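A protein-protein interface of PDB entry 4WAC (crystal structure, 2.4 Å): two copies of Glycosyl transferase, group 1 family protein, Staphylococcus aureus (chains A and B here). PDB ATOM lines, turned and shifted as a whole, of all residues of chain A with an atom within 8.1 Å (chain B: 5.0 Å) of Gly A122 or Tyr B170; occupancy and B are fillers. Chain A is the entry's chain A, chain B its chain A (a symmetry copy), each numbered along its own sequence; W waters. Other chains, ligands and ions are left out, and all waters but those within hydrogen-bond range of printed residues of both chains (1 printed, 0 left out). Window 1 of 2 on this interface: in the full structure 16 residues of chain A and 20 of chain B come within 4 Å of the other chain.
The side-chain hydroxyl (OH) of Tyr B174 sits at hydrogen-bond distance from the backbone carbonyl oxygen (O) of Thr A121, at 2.7 Å. The backbone carbonyl oxygen (O) of Gly A122 sits at hydrogen-bond distance from the side-chain hydroxyl (OH) of Tyr B170 (2.6 Å). The side-chain hydroxyl of Thr A123 lies within hydrogen-bond range of the side-chain amino group of Lys B159 (3.2 Å). The backbone NH of Tyr A124 sits at hydrogen-bond distance from the side-chain hydroxyl of Tyr B170 (3.5 Å). ND2 of Asn A143 is in hydrogen-bond range of O of Cys B169 (3.5 Å). OD1 of Asn B185 is in hydrogen-bond range of ND2 of Asn A143, 3.1 Å away. The side-chain amino group (NZ) of Lys A144 lies within hydrogen-bond range of the side-chain sulfur (SG) of Cys B169.
The backbone carbonyl oxygen (O) of Asn A103 lies within hydrogen-bond range of the backbone NH (N) of Ile A119, at 2.8 Å. The side-chain amide nitrogen (ND2) of Asn A103 sits at hydrogen-bond distance from the side-chain hydroxyl (OG1) of Thr A120 (3.1 Å). The side-chain carboxylate (OD2) of Asp A118 is in hydrogen-bond range of the backbone NH (N) of Thr A120 (2.8 Å). The side-chain hydroxyl of Thr A123 is in hydrogen-bond range of the side-chain hydroxyl of Thr A121, at 3.1 Å. N of Val B172 is in hydrogen-bond range of O of Lys B159, 2.8 Å away. The backbone NH (N) of Thr B161 lies within hydrogen-bond range of the backbone carbonyl oxygen (O) of Tyr B170 (2.9 Å).
CD1 of Ile A105 touches O of Leu B199, at 3.8 Å. Tyr B170 touches Phe A117. Leu B199 touches Phe A117. Pro B180 touches Ile A119. CE2 of Tyr B174 touches O of Thr A120, at 3.9 Å. CD of Pro B180 touches O of Thr A120, 3.6 Å away. Thr A121 touches Lys B159. OH of Tyr B170 touches C of Thr A123, 3.9 Å away. Thr B161 touches Asp A142 (CG2 to CA, 3.7 Å). O of Asp A142 touches SG of Cys B169 (3.9 Å).
Asn A103 touches none of the printed residues of chain B. Printed residues of chain B within 4 Å of Phe A117: Tyr B170 (3.4 Å), Ser B183 (3.8 Å) and Leu B199 (3.7 Å). Of the printed residues of chain B, Thr A120 touches Tyr B174 (3.9 Å) and Pro B180 (3.6 Å). Of chain B, only Tyr B170, Val B172 and Pro B180 come within 4 Å of Gly A122. Of chain A, only Asp A142, Asn A143 and Lys A144 come within 4 Å of Cys B169. Of chain A, only Phe A117 (3.4 Å), Gly A122 (2.6 Å), Thr A123 (3.9 Å), Tyr A124 (3.5 Å) and Asn A143 (3.4 Å) come within 4 Å of Tyr B170. Gln B171 touches none of the printed residues of chain A.
Of the 15 printed residues of chain A, 11 touch a printed residue of chain B. Of the 15 printed residues of chain B, 10 touch a printed residue of chain A. Hydrophobic or aromatic side chains of chain B that line the printed part of chain A: Tyr B170, Val B172, Tyr B174, Pro B180 and Leu B199. Among the printed residues, 22 pairs touch across the chains.
No position is printed for both chains.
Water W1 bridges the side-chain amide oxygen of Asn B185 (2.7 Å) and the side-chain amide oxygen of Asn A143 (3.0 Å).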
ATOM      1  N   ASN A 103       9.001  19.932  20.517  1.00  0.00           N
ATOM      2  CA  ASN A 103       8.495  21.084  21.260  1.00  0.00           C
ATOM      3  C   ASN A 103       7.505  20.692  22.367  1.00  0.00           C
ATOM      4  O   ASN A 103       6.532  21.428  22.637  1.00  0.00           O
ATOM      5  CB  ASN A 103       7.832  22.089  20.297  1.00  0.00           C
ATOM      6  CG  ASN A 103       7.766  23.519  20.875  1.00  0.00           C
ATOM      7  OD1 ASN A 103       8.804  24.131  21.136  1.00  0.00           O
ATOM      8  ND2 ASN A 103       6.540  24.069  21.031  1.00  0.00           N
ATOM      9  N   ILE A 105       7.004  19.195  26.546  1.00  0.00           N
ATOM     10  CA  ILE A 105       7.499  18.648  27.794  1.00  0.00           C
ATOM     11  C   ILE A 105       6.734  17.403  28.172  1.00  0.00           C
ATOM     12  O   ILE A 105       5.544  17.226  27.815  1.00  0.00           O
ATOM     13  CB  ILE A 105       7.369  19.615  28.930  1.00  0.00           C
ATOM     14  CG1 ILE A 105       6.045  20.345  28.819  1.00  0.00           C
ATOM     15  CG2 ILE A 105       8.544  20.583  28.975  1.00  0.00           C
ATOM     16  CD1 ILE A 105       5.612  20.861  30.191  1.00  0.00           C
ATOM     17  N   TYR A 116       2.409  14.473  27.050  1.00  0.00           N
ATOM     18  CA  TYR A 116       3.260  15.455  26.388  1.00  0.00           C
ATOM     19  C   TYR A 116       2.479  16.721  26.012  1.00  0.00           C
ATOM     20  O   TYR A 116       1.414  16.660  25.390  1.00  0.00           O
ATOM     21  CB  TYR A 116       3.921  14.807  25.154  1.00  0.00           C
ATOM     22  CG  TYR A 116       4.856  13.659  25.527  1.00  0.00           C
ATOM     23  CD1 TYR A 116       4.369  12.367  25.789  1.00  0.00           C
ATOM     24  CD2 TYR A 116       6.225  13.875  25.645  1.00  0.00           C
ATOM     25  CE1 TYR A 116       5.258  11.301  26.161  1.00  0.00           C
ATOM     26  CE2 TYR A 116       7.099  12.849  26.016  1.00  0.00           C
ATOM     27  CZ  TYR A 116       6.622  11.561  26.261  1.00  0.00           C
ATOM     28  OH  TYR A 116       7.526  10.585  26.628  1.00  0.00           O
ATOM     29  N   PHE A 117       3.024  17.876  26.382  1.00  0.00           N
ATOM     30  CA  PHE A 117       2.341  19.148  26.231  1.00  0.00           C
ATOM     31  C   PHE A 117       3.214  20.109  25.464  1.00  0.00           C
ATOM     32  O   PHE A 117       4.406  20.204  25.737  1.00  0.00           O
ATOM     33  CB  PHE A 117       1.983  19.739  27.601  1.00  0.00           C
ATOM     34  CG  PHE A 117       1.035  18.900  28.400  1.00  0.00           C
ATOM     35  CD1 PHE A 117       1.501  17.827  29.165  1.00  0.00           C
ATOM     36  CD2 PHE A 117      -0.346  19.171  28.385  1.00  0.00           C
ATOM     37  CE1 PHE A 117       0.609  17.030  29.897  1.00  0.00           C
ATOM     38  CE2 PHE A 117      -1.249  18.378  29.138  1.00  0.00           C
ATOM     39  CZ  PHE A 117      -0.766  17.303  29.894  1.00  0.00           C
ATOM     40  N   ASP A 118       2.632  20.823  24.499  1.00  0.00           N
ATOM     41  CA  ASP A 118       3.409  21.773  23.706  1.00  0.00           C
ATOM     42  C   ASP A 118       4.004  22.863  24.609  1.00  0.00           C
ATOM     43  O   ASP A 118       3.265  23.476  25.394  1.00  0.00           O
ATOM     44  CB  ASP A 118       2.524  22.437  22.634  1.00  0.00           C
ATOM     45  CG  ASP A 118       3.316  23.389  21.753  1.00  0.00           C
ATOM     46  OD1 ASP A 118       3.892  22.944  20.736  1.00  0.00           O
ATOM     47  OD2 ASP A 118       3.415  24.579  22.113  1.00  0.00           O
ATOM     48  N   ILE A 119       5.293  23.171  24.482  1.00  0.00           N
ATOM     49  CA  ILE A 119       5.848  24.097  25.456  1.00  0.00           C
ATOM     50  C   ILE A 119       5.547  25.558  25.122  1.00  0.00           C
ATOM     51  O   ILE A 119       5.716  26.430  25.971  1.00  0.00           O
ATOM     52  CB  ILE A 119       7.369  23.927  25.643  1.00  0.00           C
ATOM     53  CG1 ILE A 119       8.164  24.376  24.424  1.00  0.00           C
ATOM     54  CG2 ILE A 119       7.729  22.498  25.994  1.00  0.00           C
ATOM     55  CD1 ILE A 119       9.646  24.065  24.638  1.00  0.00           C
ATOM     56  N   THR A 120       5.110  25.839  23.910  1.00  0.00           N
ATOM     57  CA  THR A 120       4.734  27.209  23.527  1.00  0.00           C
ATOM     58  C   THR A 120       3.295  27.554  23.891  1.00  0.00           C
ATOM     59  O   THR A 120       3.018  28.662  24.345  1.00  0.00           O
ATOM     60  CB  THR A 120       4.908  27.406  22.009  1.00  0.00           C
ATOM     61  OG1 THR A 120       6.267  27.080  21.680  1.00  0.00           O
ATOM     62  CG2 THR A 120       4.560  28.859  21.576  1.00  0.00           C
ATOM     63  N   THR A 121       2.378  26.607  23.690  1.00  0.00           N
ATOM     64  CA  THR A 121       0.964  26.869  23.903  1.00  0.00           C
ATOM     65  C   THR A 121       0.333  26.132  25.066  1.00  0.00           C
ATOM     66  O   THR A 121      -0.748  26.544  25.527  1.00  0.00           O
ATOM     67  CB  THR A 121       0.144  26.508  22.651  1.00  0.00           C
ATOM     68  OG1 THR A 121       0.256  25.107  22.417  1.00  0.00           O
ATOM     69  CG2 THR A 121       0.663  27.266  21.396  1.00  0.00           C
ATOM     70  N   GLY A 122       0.967  25.046  25.532  1.00  0.00           N
ATOM     71  CA  GLY A 122       0.424  24.241  26.622  1.00  0.00           C
ATOM     72  C   GLY A 122      -0.628  23.242  26.146  1.00  0.00           C
ATOM     73  O   GLY A 122      -1.235  22.532  26.963  1.00  0.00           O
ATOM     74  N   THR A 123      -0.872  23.172  24.834  1.00  0.00           N
ATOM     75  CA  THR A 123      -1.830  22.181  24.307  1.00  0.00           C
ATOM     76  C   THR A 123      -1.439  20.722  24.614  1.00  0.00           C
ATOM     77  O   THR A 123      -0.256  20.362  24.609  1.00  0.00           O
ATOM     78  CB  THR A 123      -2.000  22.386  22.796  1.00  0.00           C
ATOM     79  OG1 THR A 123      -2.544  23.687  22.625  1.00  0.00           O
ATOM     80  CG2 THR A 123      -2.926  21.319  22.109  1.00  0.00           C
ATOM     81  N   TYR A 124      -2.446  19.912  24.936  1.00  0.00           N
ATOM     82  CA  TYR A 124      -2.248  18.476  25.180  1.00  0.00           C
ATOM     83  C   TYR A 124      -1.936  17.775  23.861  1.00  0.00           C
ATOM     84  O   TYR A 124      -2.755  17.797  22.958  1.00  0.00           O
ATOM     85  CB  TYR A 124      -3.489  17.876  25.805  1.00  0.00           C
ATOM     86  CG  TYR A 124      -3.396  16.414  26.209  1.00  0.00           C
ATOM     87  CD1 TYR A 124      -2.175  15.824  26.533  1.00  0.00           C
ATOM     88  CD2 TYR A 124      -4.547  15.617  26.276  1.00  0.00           C
ATOM     89  CE1 TYR A 124      -2.092  14.501  26.906  1.00  0.00           C
ATOM     90  CE2 TYR A 124      -4.470  14.279  26.670  1.00  0.00           C
ATOM     91  CZ  TYR A 124      -3.231  13.738  26.969  1.00  0.00           C
ATOM     92  OH  TYR A 124      -3.110  12.439  27.372  1.00  0.00           O
ATOM     93  N   ILE A 125      -0.767  17.153  23.745  1.00  0.00           N
ATOM     94  CA  ILE A 125      -0.370  16.569  22.462  1.00  0.00           C
ATOM     95  C   ILE A 125      -0.485  15.052  22.428  1.00  0.00           C
ATOM     96  O   ILE A 125      -1.059  14.495  21.482  1.00  0.00           O
ATOM     97  CB  ILE A 125       1.079  16.929  22.109  1.00  0.00           C
ATOM     98  CG1 ILE A 125       1.221  18.448  22.021  1.00  0.00           C
ATOM     99  CG2 ILE A 125       1.528  16.195  20.808  1.00  0.00           C
ATOM    100  CD1 ILE A 125       0.399  19.088  20.835  1.00  0.00           C
ATOM    101  N   ASP A 142      -7.861  19.255  19.938  1.00  0.00           N
ATOM    102  CA  ASP A 142      -8.810  19.921  20.835  1.00  0.00           C
ATOM    103  C   ASP A 142      -9.085  19.080  22.087  1.00  0.00           C
ATOM    104  O   ASP A 142     -10.234  18.980  22.549  1.00  0.00           O
ATOM    105  CB  ASP A 142     -10.123  20.224  20.084  1.00  0.00           C
ATOM    106  CG  ASP A 142      -9.863  20.853  18.699  1.00  0.00           C
ATOM    107  OD1 ASP A 142      -8.857  21.579  18.559  1.00  0.00           O
ATOM    108  OD2 ASP A 142     -10.624  20.584  17.735  1.00  0.00           O
ATOM    109  N   ASN A 143      -8.021  18.473  22.634  1.00  0.00           N
ATOM    110  CA  ASN A 143      -8.083  17.737  23.889  1.00  0.00           C
ATOM    111  C   ASN A 143      -8.904  16.464  23.797  1.00  0.00           C
ATOM    112  O   ASN A 143      -9.302  15.938  24.824  1.00  0.00           O
ATOM    113  CB  ASN A 143      -8.650  18.619  25.024  1.00  0.00           C
ATOM    114  CG  ASN A 143      -7.970  18.356  26.354  1.00  0.00           C
ATOM    115  OD1 ASN A 143      -6.741  18.249  26.409  1.00  0.00           O
ATOM    116  ND2 ASN A 143      -8.756  18.216  27.420  1.00  0.00           N
ATOM    117  N   LYS A 144      -9.161  15.984  22.579  1.00  0.00           N
ATOM    118  CA  LYS A 144      -9.852  14.696  22.354  1.00  0.00           C
ATOM    119  C   LYS A 144      -8.926  13.792  21.544  1.00  0.00           C
ATOM    120  O   LYS A 144      -8.268  14.259  20.589  1.00  0.00           O
ATOM    121  CB  LYS A 144     -11.167  14.857  21.591  1.00  0.00           C
ATOM    122  CG  LYS A 144     -12.233  15.716  22.215  1.00  0.00           C
ATOM    123  CD  LYS A 144     -12.710  15.128  23.511  1.00  0.00           C
ATOM    124  CE  LYS A 144     -13.977  15.803  24.022  1.00  0.00           C
ATOM    125  NZ  LYS A 144     -13.795  17.237  24.381  1.00  0.00           N
ATOM    126  N   LYS B 159      -5.818  30.555  27.524  1.00  0.00           N
ATOM    127  CA  LYS B 159      -6.325  29.920  26.300  1.00  0.00           C
ATOM    128  C   LYS B 159      -7.332  28.870  26.675  1.00  0.00           C
ATOM    129  O   LYS B 159      -7.054  28.018  27.540  1.00  0.00           O
ATOM    130  CB  LYS B 159      -5.219  29.264  25.476  1.00  0.00           C
ATOM    131  CG  LYS B 159      -5.775  28.571  24.219  1.00  0.00           C
ATOM    132  CD  LYS B 159      -4.673  28.010  23.292  1.00  0.00           C
ATOM    133  CE  LYS B 159      -4.088  26.642  23.775  1.00  0.00           C
ATOM    134  NZ  LYS B 159      -5.005  25.460  23.543  1.00  0.00           N
ATOM    135  N   GLU B 160      -8.487  28.913  26.019  1.00  0.00           N
ATOM    136  CA  GLU B 160      -9.523  27.931  26.248  1.00  0.00           C
ATOM    137  C   GLU B 160      -9.834  27.088  25.007  1.00  0.00           C
ATOM    138  O   GLU B 160      -9.814  27.579  23.868  1.00  0.00           O
ATOM    139  CB  GLU B 160     -10.799  28.608  26.730  1.00  0.00           C
ATOM    140  CG  GLU B 160     -10.655  29.131  28.139  1.00  0.00           C
ATOM    141  CD  GLU B 160     -11.851  29.985  28.534  1.00  0.00           C
ATOM    142  OE1 GLU B 160     -12.113  30.985  27.815  1.00  0.00           O
ATOM    143  OE2 GLU B 160     -12.543  29.620  29.521  1.00  0.00           O
ATOM    144  N   THR B 161     -10.153  25.824  25.238  1.00  0.00           N
ATOM    145  CA  THR B 161     -10.485  24.931  24.153  1.00  0.00           C
ATOM    146  C   THR B 161     -11.946  24.541  24.228  1.00  0.00           C
ATOM    147  O   THR B 161     -12.476  24.251  25.310  1.00  0.00           O
ATOM    148  CB  THR B 161      -9.597  23.691  24.206  1.00  0.00           C
ATOM    149  OG1 THR B 161      -8.237  24.116  24.118  1.00  0.00           O
ATOM    150  CG2 THR B 161      -9.912  22.675  23.051  1.00  0.00           C
ATOM    151  N   VAL B 168     -16.311  24.910  27.043  1.00  0.00           N
ATOM    152  CA  VAL B 168     -14.904  24.732  27.458  1.00  0.00           C
ATOM    153  C   VAL B 168     -14.598  23.334  28.019  1.00  0.00           C
ATOM    154  O   VAL B 168     -15.322  22.845  28.891  1.00  0.00           O
ATOM    155  CB  VAL B 168     -14.498  25.791  28.523  1.00  0.00           C
ATOM    156  CG1 VAL B 168     -13.034  25.609  28.928  1.00  0.00           C
ATOM    157  CG2 VAL B 168     -14.737  27.220  27.942  1.00  0.00           C
ATOM    158  N   CYS B 169     -13.536  22.697  27.516  1.00  0.00           N
ATOM    159  CA  CYS B 169     -13.120  21.361  28.007  1.00  0.00           C
ATOM    160  C   CYS B 169     -11.643  21.364  28.370  1.00  0.00           C
ATOM    161  O   CYS B 169     -11.132  20.349  28.839  1.00  0.00           O
ATOM    162  CB  CYS B 169     -13.380  20.233  26.955  1.00  0.00           C
ATOM    163  SG  CYS B 169     -12.486  20.488  25.373  1.00  0.00           S
ATOM    164  N   TYR B 170     -10.963  22.498  28.176  1.00  0.00           N
ATOM    165  CA  TYR B 170      -9.537  22.578  28.554  1.00  0.00           C
ATOM    166  C   TYR B 170      -9.104  24.012  28.716  1.00  0.00           C
ATOM    167  O   TYR B 170      -9.557  24.882  27.956  1.00  0.00           O
ATOM    168  CB  TYR B 170      -8.681  21.891  27.500  1.00  0.00           C
ATOM    169  CG  TYR B 170      -7.180  21.712  27.724  1.00  0.00           C
ATOM    170  CD1 TYR B 170      -6.679  20.769  28.627  1.00  0.00           C
ATOM    171  CD2 TYR B 170      -6.258  22.435  26.949  1.00  0.00           C
ATOM    172  CE1 TYR B 170      -5.316  20.580  28.774  1.00  0.00           C
ATOM    173  CE2 TYR B 170      -4.884  22.241  27.086  1.00  0.00           C
ATOM    174  CZ  TYR B 170      -4.431  21.310  28.002  1.00  0.00           C
ATOM    175  OH  TYR B 170      -3.092  21.097  28.155  1.00  0.00           O
ATOM    176  N   GLN B 171      -8.215  24.280  29.672  1.00  0.00           N
ATOM    177  CA  GLN B 171      -7.728  25.644  29.846  1.00  0.00           C
ATOM    178  C   GLN B 171      -6.208  25.653  30.022  1.00  0.00           C
ATOM    179  O   GLN B 171      -5.633  24.749  30.644  1.00  0.00           O
ATOM    180  CB  GLN B 171      -8.363  26.309  31.078  1.00  0.00           C
ATOM    181  CG  GLN B 171      -9.846  26.436  31.025  1.00  0.00           C
ATOM    182  CD  GLN B 171     -10.425  26.991  32.344  1.00  0.00           C
ATOM    183  OE1 GLN B 171      -9.991  26.613  33.422  1.00  0.00           O
ATOM    184  NE2 GLN B 171     -11.339  27.950  32.244  1.00  0.00           N
ATOM    185  N   VAL B 172      -5.578  26.707  29.496  1.00  0.00           N
ATOM    186  CA  VAL B 172      -4.174  26.959  29.759  1.00  0.00           C
ATOM    187  C   VAL B 172      -3.991  28.376  30.345  1.00  0.00           C
ATOM    188  O   VAL B 172      -4.649  29.316  29.895  1.00  0.00           O
ATOM    189  CB  VAL B 172      -3.346  26.816  28.486  1.00  0.00           C
ATOM    190  CG1 VAL B 172      -1.828  27.042  28.770  1.00  0.00           C
ATOM    191  CG2 VAL B 172      -3.615  25.437  27.824  1.00  0.00           C
ATOM    192  N   TYR B 174      -1.187  31.468  31.128  1.00  0.00           N
ATOM    193  CA  TYR B 174       0.156  31.867  30.746  1.00  0.00           C
ATOM    194  C   TYR B 174       0.728  32.890  31.727  1.00  0.00           C
ATOM    195  O   TYR B 174      -0.003  33.697  32.300  1.00  0.00           O
ATOM    196  CB  TYR B 174       0.167  32.473  29.331  1.00  0.00           C
ATOM    197  CG  TYR B 174      -0.356  31.558  28.266  1.00  0.00           C
ATOM    198  CD1 TYR B 174      -1.730  31.488  28.002  1.00  0.00           C
ATOM    199  CD2 TYR B 174       0.509  30.767  27.516  1.00  0.00           C
ATOM    200  CE1 TYR B 174      -2.218  30.670  27.022  1.00  0.00           C
ATOM    201  CE2 TYR B 174       0.026  29.920  26.527  1.00  0.00           C
ATOM    202  CZ  TYR B 174      -1.335  29.877  26.290  1.00  0.00           C
ATOM    203  OH  TYR B 174      -1.840  29.017  25.345  1.00  0.00           O
ATOM    204  N   PRO B 180       3.174  29.112  29.107  1.00  0.00           N
ATOM    205  CA  PRO B 180       2.149  28.281  29.771  1.00  0.00           C
ATOM    206  C   PRO B 180       2.727  27.696  31.064  1.00  0.00           C
ATOM    207  O   PRO B 180       3.861  27.209  31.035  1.00  0.00           O
ATOM    208  CB  PRO B 180       1.842  27.193  28.726  1.00  0.00           C
ATOM    209  CG  PRO B 180       3.164  27.061  27.900  1.00  0.00           C
ATOM    210  CD  PRO B 180       3.660  28.524  27.834  1.00  0.00           C
ATOM    211  N   SER B 183      -2.000  23.849  32.854  1.00  0.00           N
ATOM    212  CA  SER B 183      -3.148  23.535  32.033  1.00  0.00           C
ATOM    213  C   SER B 183      -4.025  22.560  32.781  1.00  0.00           C
ATOM    214  O   SER B 183      -3.537  21.864  33.686  1.00  0.00           O
ATOM    215  CB  SER B 183      -2.731  22.950  30.685  1.00  0.00           C
ATOM    216  OG  SER B 183      -2.302  21.619  30.910  1.00  0.00           O
ATOM    217  N   ARG B 184      -5.309  22.484  32.396  1.00  0.00           N
ATOM    218  CA  ARG B 184      -6.230  21.588  33.106  1.00  0.00           C
ATOM    219  C   ARG B 184      -7.465  21.170  32.318  1.00  0.00           C
ATOM    220  O   ARG B 184      -7.956  21.891  31.442  1.00  0.00           O
ATOM    221  CB  ARG B 184      -6.666  22.247  34.424  1.00  0.00           C
ATOM    222  CG  ARG B 184      -7.446  23.521  34.266  1.00  0.00           C
ATOM    223  CD  ARG B 184      -7.640  24.164  35.648  1.00  0.00           C
ATOM    224  NE  ARG B 184      -8.640  25.227  35.583  1.00  0.00           N
ATOM    225  CZ  ARG B 184      -9.157  25.839  36.643  1.00  0.00           C
ATOM    226  NH1 ARG B 184      -8.796  25.480  37.874  1.00  0.00           N
ATOM    227  NH2 ARG B 184     -10.047  26.798  36.470  1.00  0.00           N
ATOM    228  N   ASN B 185      -7.966  19.988  32.631  1.00  0.00           N
ATOM    229  CA  ASN B 185      -9.166  19.482  31.975  1.00  0.00           C
ATOM    230  C   ASN B 185     -10.407  20.059  32.611  1.00  0.00           C
ATOM    231  O   ASN B 185     -10.479  20.176  33.848  1.00  0.00           O
ATOM    232  CB  ASN B 185      -9.217  17.937  32.027  1.00  0.00           C
ATOM    233  CG  ASN B 185      -8.128  17.296  31.181  1.00  0.00           C
ATOM    234  OD1 ASN B 185      -7.626  17.923  30.238  1.00  0.00           O
ATOM    235  ND2 ASN B 185      -7.775  16.039  31.480  1.00  0.00           N
ATOM    236  N   ILE B 186     -11.384  20.394  31.777  1.00  0.00           N
ATOM    237  CA  ILE B 186     -12.722  20.785  32.236  1.00  0.00           C
ATOM    238  C   ILE B 186     -13.803  19.806  31.772  1.00  0.00           C
ATOM    239  O   ILE B 186     -13.867  19.468  30.591  1.00  0.00           O
ATOM    240  CB  ILE B 186     -13.093  22.185  31.693  1.00  0.00           C
ATOM    241  CG1 ILE B 186     -11.994  23.165  32.049  1.00  0.00           C
ATOM    242  CG2 ILE B 186     -14.428  22.674  32.269  1.00  0.00           C
ATOM    243  CD1 ILE B 186     -11.836  23.323  33.505  1.00  0.00           C
ATOM    244  N   LEU B 199       2.735  22.516  34.435  1.00  0.00           N
ATOM    245  CA  LEU B 199       3.744  22.481  33.382  1.00  0.00           C
ATOM    246  C   LEU B 199       5.092  23.032  33.846  1.00  0.00           C
ATOM    247  O   LEU B 199       6.130  22.449  33.554  1.00  0.00           O
ATOM    248  CB  LEU B 199       3.243  23.271  32.141  1.00  0.00           C
ATOM    249  CG  LEU B 199       1.877  22.837  31.577  1.00  0.00           C
ATOM    250  CD1 LEU B 199       1.322  23.815  30.574  1.00  0.00           C
ATOM    251  CD2 LEU B 199       1.938  21.437  30.957  1.00  0.00           C
HETATM  252  O   HOH W   1      -5.433  17.165  28.937  1.00  0.00           O
